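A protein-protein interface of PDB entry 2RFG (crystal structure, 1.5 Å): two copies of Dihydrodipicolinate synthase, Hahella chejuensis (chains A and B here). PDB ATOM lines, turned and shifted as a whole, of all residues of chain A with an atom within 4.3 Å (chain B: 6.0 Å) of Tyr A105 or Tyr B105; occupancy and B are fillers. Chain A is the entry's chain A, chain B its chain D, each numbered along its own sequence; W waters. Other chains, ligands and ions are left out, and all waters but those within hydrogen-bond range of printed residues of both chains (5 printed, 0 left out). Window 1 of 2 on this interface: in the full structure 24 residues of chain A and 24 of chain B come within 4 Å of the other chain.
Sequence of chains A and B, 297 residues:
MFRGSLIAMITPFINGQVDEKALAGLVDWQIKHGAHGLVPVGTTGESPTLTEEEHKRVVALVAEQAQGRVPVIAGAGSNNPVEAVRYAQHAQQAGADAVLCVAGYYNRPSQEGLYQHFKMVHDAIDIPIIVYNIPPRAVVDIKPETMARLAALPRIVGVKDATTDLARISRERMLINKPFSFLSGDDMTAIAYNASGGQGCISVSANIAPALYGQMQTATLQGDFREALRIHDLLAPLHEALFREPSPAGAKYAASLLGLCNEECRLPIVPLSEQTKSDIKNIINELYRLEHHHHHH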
ATOM      1  N   SER A  78       8.603   4.159 -16.214  1.00  0.00           N
ATOM      2  CA  SER A  78       8.975   5.561 -16.358  1.00  0.00           C
ATOM      3  C   SER A  78      10.478   5.619 -16.554  1.00  0.00           C
ATOM      4  O   SER A  78      11.187   4.689 -16.181  1.00  0.00           O
ATOM      5  CB  SER A  78       8.641   6.366 -15.097  1.00  0.00           C
ATOM      6  OG  SER A  78       8.944   7.744 -15.287  1.00  0.00           O
ATOM      7  N   ASN A  79      10.957   6.715 -17.134  1.00  0.00           N
ATOM      8  CA  ASN A  79      12.394   6.988 -17.130  1.00  0.00           C
ATOM      9  C   ASN A  79      12.862   7.747 -15.882  1.00  0.00           C
ATOM     10  O   ASN A  79      14.058   8.009 -15.714  1.00  0.00           O
ATOM     11  CB  ASN A  79      12.898   7.641 -18.435  1.00  0.00           C
ATOM     12  CG  ASN A  79      12.213   8.949 -18.780  1.00  0.00           C
ATOM     13  OD1 ASN A  79      12.480   9.527 -19.854  1.00  0.00           O
ATOM     14  ND2 ASN A  79      11.342   9.430 -17.918  1.00  0.00           N
ATOM     15  N   VAL A 102       9.735  -0.856 -17.013  1.00  0.00           N
ATOM     16  CA  VAL A 102      10.792  -0.410 -17.914  1.00  0.00           C
ATOM     17  C   VAL A 102      11.509   0.777 -17.265  1.00  0.00           C
ATOM     18  O   VAL A 102      10.928   1.464 -16.405  1.00  0.00           O
ATOM     19  CB  VAL A 102      10.200   0.004 -19.296  1.00  0.00           C
ATOM     20  CG1 VAL A 102       9.458   1.354 -19.219  1.00  0.00           C
ATOM     21  CG2 VAL A 102      11.289   0.034 -20.363  1.00  0.00           C
ATOM     22  N   ALA A 103      12.752   1.023 -17.680  1.00  0.00           N
ATOM     23  CA  ALA A 103      13.536   2.155 -17.163  1.00  0.00           C
ATOM     24  C   ALA A 103      14.406   2.734 -18.265  1.00  0.00           C
ATOM     25  O   ALA A 103      14.721   2.046 -19.242  1.00  0.00           O
ATOM     26  CB  ALA A 103      14.427   1.690 -16.014  1.00  0.00           C
ATOM     27  N   GLY A 104      14.806   3.994 -18.097  1.00  0.00           N
ATOM     28  CA  GLY A 104      15.949   4.535 -18.832  1.00  0.00           C
ATOM     29  C   GLY A 104      15.743   4.941 -20.279  1.00  0.00           C
ATOM     30  O   GLY A 104      16.710   5.298 -20.957  1.00  0.00           O
ATOM     31  N   TYR A 105      14.509   4.889 -20.779  1.00  0.00           N
ATOM     32  CA  TYR A 105      14.298   5.399 -22.137  1.00  0.00           C
ATOM     33  C   TYR A 105      14.543   6.905 -22.199  1.00  0.00           C
ATOM     34  O   TYR A 105      14.212   7.646 -21.271  1.00  0.00           O
ATOM     35  CB  TYR A 105      12.902   5.046 -22.686  1.00  0.00           C
ATOM     36  CG  TYR A 105      11.735   5.493 -21.842  1.00  0.00           C
ATOM     37  CD1 TYR A 105      11.225   6.792 -21.946  1.00  0.00           C
ATOM     38  CD2 TYR A 105      11.116   4.609 -20.965  1.00  0.00           C
ATOM     39  CE1 TYR A 105      10.143   7.208 -21.181  1.00  0.00           C
ATOM     40  CE2 TYR A 105      10.017   5.018 -20.187  1.00  0.00           C
ATOM     41  CZ  TYR A 105       9.540   6.321 -20.308  1.00  0.00           C
ATOM     42  OH  TYR A 105       8.462   6.756 -19.551  1.00  0.00           O
ATOM     43  N   TYR A 106      15.154   7.334 -23.300  1.00  0.00           N
ATOM     44  CA  TYR A 106      15.433   8.732 -23.599  1.00  0.00           C
ATOM     45  C   TYR A 106      16.602   9.334 -22.801  1.00  0.00           C
ATOM     46  O   TYR A 106      17.561   9.842 -23.409  1.00  0.00           O
ATOM     47  CB  TYR A 106      14.165   9.609 -23.570  1.00  0.00           C
ATOM     48  CG  TYR A 106      14.380  11.004 -24.111  1.00  0.00           C
ATOM     49  CD1 TYR A 106      14.921  11.198 -25.383  1.00  0.00           C
ATOM     50  CD2 TYR A 106      14.038  12.121 -23.357  1.00  0.00           C
ATOM     51  CE1 TYR A 106      15.136  12.476 -25.879  1.00  0.00           C
ATOM     52  CE2 TYR A 106      14.235  13.407 -23.847  1.00  0.00           C
ATOM     53  CZ  TYR A 106      14.799  13.571 -25.101  1.00  0.00           C
ATOM     54  OH  TYR A 106      15.002  14.858 -25.580  1.00  0.00           O
ATOM     55  N   ASN A 107      16.568   9.257 -21.468  1.00  0.00           N
ATOM     56  CA  ASN A 107      17.744   9.704 -20.699  1.00  0.00           C
ATOM     57  C   ASN A 107      18.962   8.769 -20.765  1.00  0.00           C
ATOM     58  O   ASN A 107      20.088   9.215 -20.546  1.00  0.00           O
ATOM     59  CB  ASN A 107      17.396  10.124 -19.252  1.00  0.00           C
ATOM     60  CG  ASN A 107      16.594   9.084 -18.487  1.00  0.00           C
ATOM     61  OD1 ASN A 107      16.433   7.935 -18.914  1.00  0.00           O
ATOM     62  ND2 ASN A 107      16.069   9.502 -17.327  1.00  0.00           N
ATOM     63  N   ALA A 138      13.618   1.587 -25.977  1.00  0.00           N
ATOM     64  CA  ALA A 138      14.270   2.363 -24.908  1.00  0.00           C
ATOM     65  C   ALA A 138      15.739   2.660 -25.152  1.00  0.00           C
ATOM     66  O   ALA A 138      16.334   3.481 -24.436  1.00  0.00           O
ATOM     67  CB  ALA A 138      14.111   1.651 -23.570  1.00  0.00           C
ATOM     68  N   PRO B  48      13.706  14.799 -17.968  1.00  0.00           N
ATOM     69  CA  PRO B  48      12.924  13.603 -17.566  1.00  0.00           C
ATOM     70  C   PRO B  48      12.677  13.428 -16.068  1.00  0.00           C
ATOM     71  O   PRO B  48      11.692  12.766 -15.693  1.00  0.00           O
ATOM     72  CB  PRO B  48      13.777  12.435 -18.088  1.00  0.00           C
ATOM     73  CG  PRO B  48      14.573  13.028 -19.213  1.00  0.00           C
ATOM     74  CD  PRO B  48      14.930  14.414 -18.699  1.00  0.00           C
ATOM     75  N   GLY B  77       9.864  19.126 -24.494  1.00  0.00           N
ATOM     76  CA  GLY B  77       9.884  17.764 -25.014  1.00  0.00           C
ATOM     77  C   GLY B  77       8.920  16.876 -24.258  1.00  0.00           C
ATOM     78  O   GLY B  77       8.723  17.042 -23.057  1.00  0.00           O
ATOM     79  N   SER B  78       8.310  15.938 -24.984  1.00  0.00           N
ATOM     80  CA  SER B  78       7.534  14.853 -24.388  1.00  0.00           C
ATOM     81  C   SER B  78       7.205  13.874 -25.487  1.00  0.00           C
ATOM     82  O   SER B  78       7.212  14.237 -26.664  1.00  0.00           O
ATOM     83  CB  SER B  78       6.223  15.345 -23.765  1.00  0.00           C
ATOM     84  OG  SER B  78       5.522  14.276 -23.133  1.00  0.00           O
ATOM     85  N   ASN B  79       6.929  12.629 -25.105  1.00  0.00           N
ATOM     86  CA  ASN B  79       6.348  11.689 -26.058  1.00  0.00           C
ATOM     87  C   ASN B  79       4.820  11.771 -26.124  1.00  0.00           C
ATOM     88  O   ASN B  79       4.188  11.090 -26.926  1.00  0.00           O
ATOM     89  CB  ASN B  79       6.876  10.251 -25.859  1.00  0.00           C
ATOM     90  CG  ASN B  79       6.599   9.672 -24.476  1.00  0.00           C
ATOM     91  OD1 ASN B  79       7.044   8.549 -24.167  1.00  0.00           O
ATOM     92  ND2 ASN B  79       5.906  10.402 -23.646  1.00  0.00           N
ATOM     93  N   ASN B  80       4.243  12.649 -25.302  1.00  0.00           N
ATOM     94  CA  ASN B  80       2.813  12.924 -25.310  1.00  0.00           C
ATOM     95  C   ASN B  80       2.599  14.383 -25.732  1.00  0.00           C
ATOM     96  O   ASN B  80       2.971  15.292 -24.979  1.00  0.00           O
ATOM     97  CB  ASN B  80       2.231  12.692 -23.913  1.00  0.00           C
ATOM     98  CG  ASN B  80       0.760  13.056 -23.828  1.00  0.00           C
ATOM     99  OD1 ASN B  80       0.136  13.397 -24.849  1.00  0.00           O
ATOM    100  ND2 ASN B  80       0.192  12.988 -22.618  1.00  0.00           N
ATOM    101  N   GLU B  83       1.134  16.869 -23.188  1.00  0.00           N
ATOM    102  CA  GLU B  83       2.096  17.338 -22.203  1.00  0.00           C
ATOM    103  C   GLU B  83       3.021  18.394 -22.811  1.00  0.00           C
ATOM    104  O   GLU B  83       3.295  19.434 -22.190  1.00  0.00           O
ATOM    105  CB  GLU B  83       2.899  16.162 -21.656  1.00  0.00           C
ATOM    106  CG  GLU B  83       3.732  16.486 -20.435  1.00  0.00           C
ATOM    107  CD  GLU B  83       4.405  15.256 -19.868  1.00  0.00           C
ATOM    108  OE1 GLU B  83       5.253  14.654 -20.569  1.00  0.00           O
ATOM    109  OE2 GLU B  83       4.085  14.895 -18.715  1.00  0.00           O
ATOM    110  N   VAL B 102      11.381  17.614 -28.800  1.00  0.00           N
ATOM    111  CA  VAL B 102      11.507  16.219 -29.219  1.00  0.00           C
ATOM    112  C   VAL B 102      10.122  15.559 -29.130  1.00  0.00           C
ATOM    113  O   VAL B 102       9.262  16.015 -28.371  1.00  0.00           O
ATOM    114  CB  VAL B 102      12.529  15.453 -28.337  1.00  0.00           C
ATOM    115  CG1 VAL B 102      11.946  15.163 -26.950  1.00  0.00           C
ATOM    116  CG2 VAL B 102      12.970  14.153 -29.005  1.00  0.00           C
ATOM    117  N   ALA B 103       9.920  14.499 -29.906  1.00  0.00           N
ATOM    118  CA  ALA B 103       8.668  13.736 -29.877  1.00  0.00           C
ATOM    119  C   ALA B 103       8.951  12.248 -30.051  1.00  0.00           C
ATOM    120  O   ALA B 103      10.003  11.873 -30.559  1.00  0.00           O
ATOM    121  CB  ALA B 103       7.720  14.228 -30.979  1.00  0.00           C
ATOM    122  N   GLY B 104       8.009  11.406 -29.633  1.00  0.00           N
ATOM    123  CA  GLY B 104       7.959  10.028 -30.115  1.00  0.00           C
ATOM    124  C   GLY B 104       8.901   9.010 -29.506  1.00  0.00           C
ATOM    125  O   GLY B 104       8.900   7.851 -29.934  1.00  0.00           O
ATOM    126  N   TYR B 105       9.694   9.411 -28.512  1.00  0.00           N
ATOM    127  CA  TYR B 105      10.537   8.418 -27.833  1.00  0.00           C
ATOM    128  C   TYR B 105       9.664   7.408 -27.102  1.00  0.00           C
ATOM    129  O   TYR B 105       8.627   7.756 -26.533  1.00  0.00           O
ATOM    130  CB  TYR B 105      11.571   9.049 -26.890  1.00  0.00           C
ATOM    131  CG  TYR B 105      11.013   9.968 -25.826  1.00  0.00           C
ATOM    132  CD1 TYR B 105      10.549   9.462 -24.614  1.00  0.00           C
ATOM    133  CD2 TYR B 105      10.968  11.344 -26.030  1.00  0.00           C
ATOM    134  CE1 TYR B 105      10.044  10.306 -23.625  1.00  0.00           C
ATOM    135  CE2 TYR B 105      10.472  12.201 -25.047  1.00  0.00           C
ATOM    136  CZ  TYR B 105      10.000  11.670 -23.851  1.00  0.00           C
ATOM    137  OH  TYR B 105       9.496  12.504 -22.864  1.00  0.00           O
ATOM    138  N   TYR B 106      10.094   6.151 -27.150  1.00  0.00           N
ATOM    139  CA  TYR B 106       9.469   5.039 -26.445  1.00  0.00           C
ATOM    140  C   TYR B 106       8.178   4.548 -27.104  1.00  0.00           C
ATOM    141  O   TYR B 106       8.086   3.364 -27.434  1.00  0.00           O
ATOM    142  CB  TYR B 106       9.340   5.299 -24.925  1.00  0.00           C
ATOM    143  CG  TYR B 106       9.002   4.046 -24.167  1.00  0.00           C
ATOM    144  CD1 TYR B 106       9.816   2.916 -24.260  1.00  0.00           C
ATOM    145  CD2 TYR B 106       7.873   3.985 -23.351  1.00  0.00           C
ATOM    146  CE1 TYR B 106       9.501   1.747 -23.586  1.00  0.00           C
ATOM    147  CE2 TYR B 106       7.558   2.814 -22.652  1.00  0.00           C
ATOM    148  CZ  TYR B 106       8.377   1.699 -22.791  1.00  0.00           C
ATOM    149  OH  TYR B 106       8.075   0.523 -22.109  1.00  0.00           O
ATOM    150  N   ASN B 107       7.185   5.420 -27.313  1.00  0.00           N
ATOM    151  CA  ASN B 107       5.992   4.989 -28.064  1.00  0.00           C
ATOM    152  C   ASN B 107       6.203   4.771 -29.572  1.00  0.00           C
ATOM    153  O   ASN B 107       5.457   4.005 -30.203  1.00  0.00           O
ATOM    154  CB  ASN B 107       4.727   5.822 -27.765  1.00  0.00           C
ATOM    155  CG  ASN B 107       4.945   7.324 -27.859  1.00  0.00           C
ATOM    156  OD1 ASN B 107       5.983   7.809 -28.329  1.00  0.00           O
ATOM    157  ND2 ASN B 107       3.940   8.073 -27.407  1.00  0.00           N
ATOM    158  N   ARG B 108       7.236   5.416 -30.129  1.00  0.00           N
ATOM    159  CA  ARG B 108       7.712   5.094 -31.488  1.00  0.00           C
ATOM    160  C   ARG B 108       6.642   5.221 -32.581  1.00  0.00           C
ATOM    161  O   ARG B 108       6.352   4.246 -33.307  1.00  0.00           O
ATOM    162  CB  ARG B 108       8.308   3.678 -31.519  1.00  0.00           C
ATOM    163  CG  ARG B 108       9.818   3.587 -31.584  1.00  0.00           C
ATOM    164  CD  ARG B 108      10.272   2.115 -31.634  1.00  0.00           C
ATOM    165  NE  ARG B 108       9.273   1.231 -32.251  1.00  0.00           N
ATOM    166  CZ  ARG B 108       9.267  -0.100 -32.161  1.00  0.00           C
ATOM    167  NH1 ARG B 108      10.216  -0.741 -31.482  1.00  0.00           N
ATOM    168  NH2 ARG B 108       8.305  -0.797 -32.750  1.00  0.00           N
ATOM    169  N   PRO B 109       6.046   6.416 -32.730  1.00  0.00           N
ATOM    170  CA  PRO B 109       5.012   6.629 -33.739  1.00  0.00           C
ATOM    171  C   PRO B 109       5.564   6.700 -35.162  1.00  0.00           C
ATOM    172  O   PRO B 109       6.785   6.775 -35.371  1.00  0.00           O
ATOM    173  CB  PRO B 109       4.439   7.990 -33.343  1.00  0.00           C
ATOM    174  CG  PRO B 109       5.607   8.703 -32.738  1.00  0.00           C
ATOM    175  CD  PRO B 109       6.312   7.638 -31.950  1.00  0.00           C
ATOM    176  N   ARG B 137      18.655   8.640 -29.052  1.00  0.00           N
ATOM    177  CA  ARG B 137      17.925   8.543 -27.783  1.00  0.00           C
ATOM    178  C   ARG B 137      16.470   8.138 -27.972  1.00  0.00           C
ATOM    179  O   ARG B 137      15.922   7.421 -27.131  1.00  0.00           O
ATOM    180  CB  ARG B 137      17.967   9.870 -27.022  1.00  0.00           C
ATOM    181  CG  ARG B 137      19.340  10.212 -26.462  1.00  0.00           C
ATOM    182  CD  ARG B 137      19.301  11.515 -25.675  1.00  0.00           C
ATOM    183  NE  ARG B 137      20.631  11.857 -25.172  1.00  0.00           N
ATOM    184  CZ  ARG B 137      21.150  11.432 -24.021  1.00  0.00           C
ATOM    185  NH1 ARG B 137      20.452  10.645 -23.205  1.00  0.00           N
ATOM    186  NH2 ARG B 137      22.379  11.802 -23.684  1.00  0.00           N
ATOM    187  N   ALA B 138      15.851   8.620 -29.048  1.00  0.00           N
ATOM    188  CA  ALA B 138      14.400   8.498 -29.233  1.00  0.00           C
ATOM    189  C   ALA B 138      13.980   7.345 -30.152  1.00  0.00           C
ATOM    190  O   ALA B 138      12.794   7.003 -30.206  1.00  0.00           O
ATOM    191  CB  ALA B 138      13.836   9.827 -29.756  1.00  0.00           C
ATOM    192  N   VAL B 139      14.956   6.767 -30.857  1.00  0.00           N
ATOM    193  CA  VAL B 139      14.769   5.752 -31.910  1.00  0.00           C
ATOM    194  C   VAL B 139      14.097   6.312 -33.168  1.00  0.00           C
ATOM    195  O   VAL B 139      14.627   6.161 -34.278  1.00  0.00           O
ATOM    196  CB  VAL B 139      14.061   4.446 -31.425  1.00  0.00           C
ATOM    197  CG1 VAL B 139      14.099   3.386 -32.526  1.00  0.00           C
ATOM    198  CG2 VAL B 139      14.716   3.905 -30.145  1.00  0.00           C
ATOM    199  N   VAL B 140      12.946   6.965 -32.997  1.00  0.00           N
ATOM    200  CA  VAL B 140      12.288   7.625 -34.133  1.00  0.00           C
ATOM    201  C   VAL B 140      13.197   8.669 -34.766  1.00  0.00           C
ATOM    202  O   VAL B 140      14.025   9.306 -34.096  1.00  0.00           O
ATOM    203  CB  VAL B 140      10.938   8.286 -33.757  1.00  0.00           C
ATOM    204  CG1 VAL B 140       9.933   7.238 -33.392  1.00  0.00           C
ATOM    205  CG2 VAL B 140      11.107   9.307 -32.642  1.00  0.00           C
HETATM  206  O   HOH W   1       6.446   7.480 -21.584  1.00  0.00           O
HETATM  207  O   HOH W   2      11.095  12.080 -20.408  1.00  0.00           O
HETATM  208  O   HOH W   3      17.074   6.150 -24.963  1.00  0.00           O
HETATM  209  O   HOH W   4       9.927  11.660 -17.587  1.00  0.00           O
HETATM  210  O   HOH W   5      22.845  10.177 -21.146  1.00  0.00           O
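O of Tyr A106 sits at hydrogen-bond distance from NH1 of Arg B137, 3.0 Å away.
The backbone carbonyl oxygen (O) of Asn A107 sits at hydrogen-bond distance from the guanidinium group (NH1) of Arg B137, 3.0 Å away.
O of Tyr A105 lies close to OD1 of Asn A79 (2.9 Å).
The backbone carbonyl oxygen of Asn A79 sits at hydrogen-bond distance from the side-chain amide nitrogen of Asn A107, at 3.0 Å.
The side-chain amide oxygen (OD1) of Asn A107 lies close to the backbone carbonyl oxygen (O) of Gly A104.
The backbone carbonyl oxygen (O) of Tyr A105 lies close to the side-chain amide oxygen (OD1) of Asn A107 (3.3 Å).
The side-chain amide oxygen (OD1) of Asn B79 lies close to the backbone carbonyl oxygen (O) of Tyr B105.
The backbone carbonyl oxygen of Tyr B105 lies close to the side-chain amide oxygen of Asn B107.
Pro B48 touches Asn A79.
Tyr B106 touches Val A102 (OH to CG1, 3.3 Å).
Tyr B105 touches Tyr A105 (CD1 to CD1, 3.8 Å).
CD1 of Tyr A105 touches CB of Tyr B106 (3.8 Å).
Tyr A106 touches Val B102 (OH to CG1, 3.4 Å).
Tyr B105 touches Tyr A106 (CD1 to CB, 3.8 Å).
ND2 of Asn A107 touches CB of Pro B48 (3.8 Å).
Of chain B, only Tyr B105 (3.8 Å) and Tyr B106 (3.8 Å) come within 4 Å of Tyr A105.
Printed residues of chain A within 4 Å of Tyr B106: Val A102 (3.3 Å) and Tyr A105 (3.8 Å).
Printed residues of chain A within 4 Å of Pro B48: Asn A79 and Asn A107.
Printed residues of chain A within 4 Å of Arg B137: Tyr A106 and Asn A107.
Gly B77 touches none of the printed residues of chain A.
Val B139 touches none of the printed residues of chain A.
The nearest residue of chain B that does not touch Tyr A105 is Asn B79 (4.5 Å).
The nearest printed residue of chain B that does not touch Val A102 is Asn B79 (9.1 Å).
Of the 9 printed residues of chain A, 5 touch a printed residue of chain B.
Along chain A the printed residues that touch a printed residue of chain B span positions 79 to 107.
Of the 18 printed residues of chain B, 5 touch a printed residue of chain A.
Among the printed residues, 9 pairs touch across the chains.
Val A102 touches Tyr B106, and with the chains exchanged Tyr A106 touches Val B102.
Tyr A105 touches its own counterpart, Tyr B105.
Tyr A105 touches Tyr B106, and with the chains exchanged Tyr A106 touches Tyr B105.
9 positions are printed for both chains.
Of the 9 pairs that touch across the chains among the printed residues, 5 have their exchanged pair printed and touching as well.
Water W4 lies within hydrogen-bond range of ND2 of Asn A79 (2.7 Å) and O of Pro B48 (2.8 Å).
Water W3 lies within hydrogen-bond range of the backbone carbonyl oxygen (O) of Arg B137 (2.8 Å), the backbone NH (N) of Tyr A106 (2.8 Å) and the backbone carbonyl oxygen (O) of Ala A138 (2.8 Å).
Water W1 lies within hydrogen-bond range of the side-chain amide oxygen (OD1) of Asn B79 (2.9 Å) and the side-chain hydroxyl (OH) of Tyr A105 (3.0 Å).
Water W2 bridges OD1 of Asn A79 (3.0 Å) and OH of Tyr B105 (3.0 Å).
Water W5 bridges O of Asn A107 (3.0 Å) and NH2 of Arg B137 (3.0 Å).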
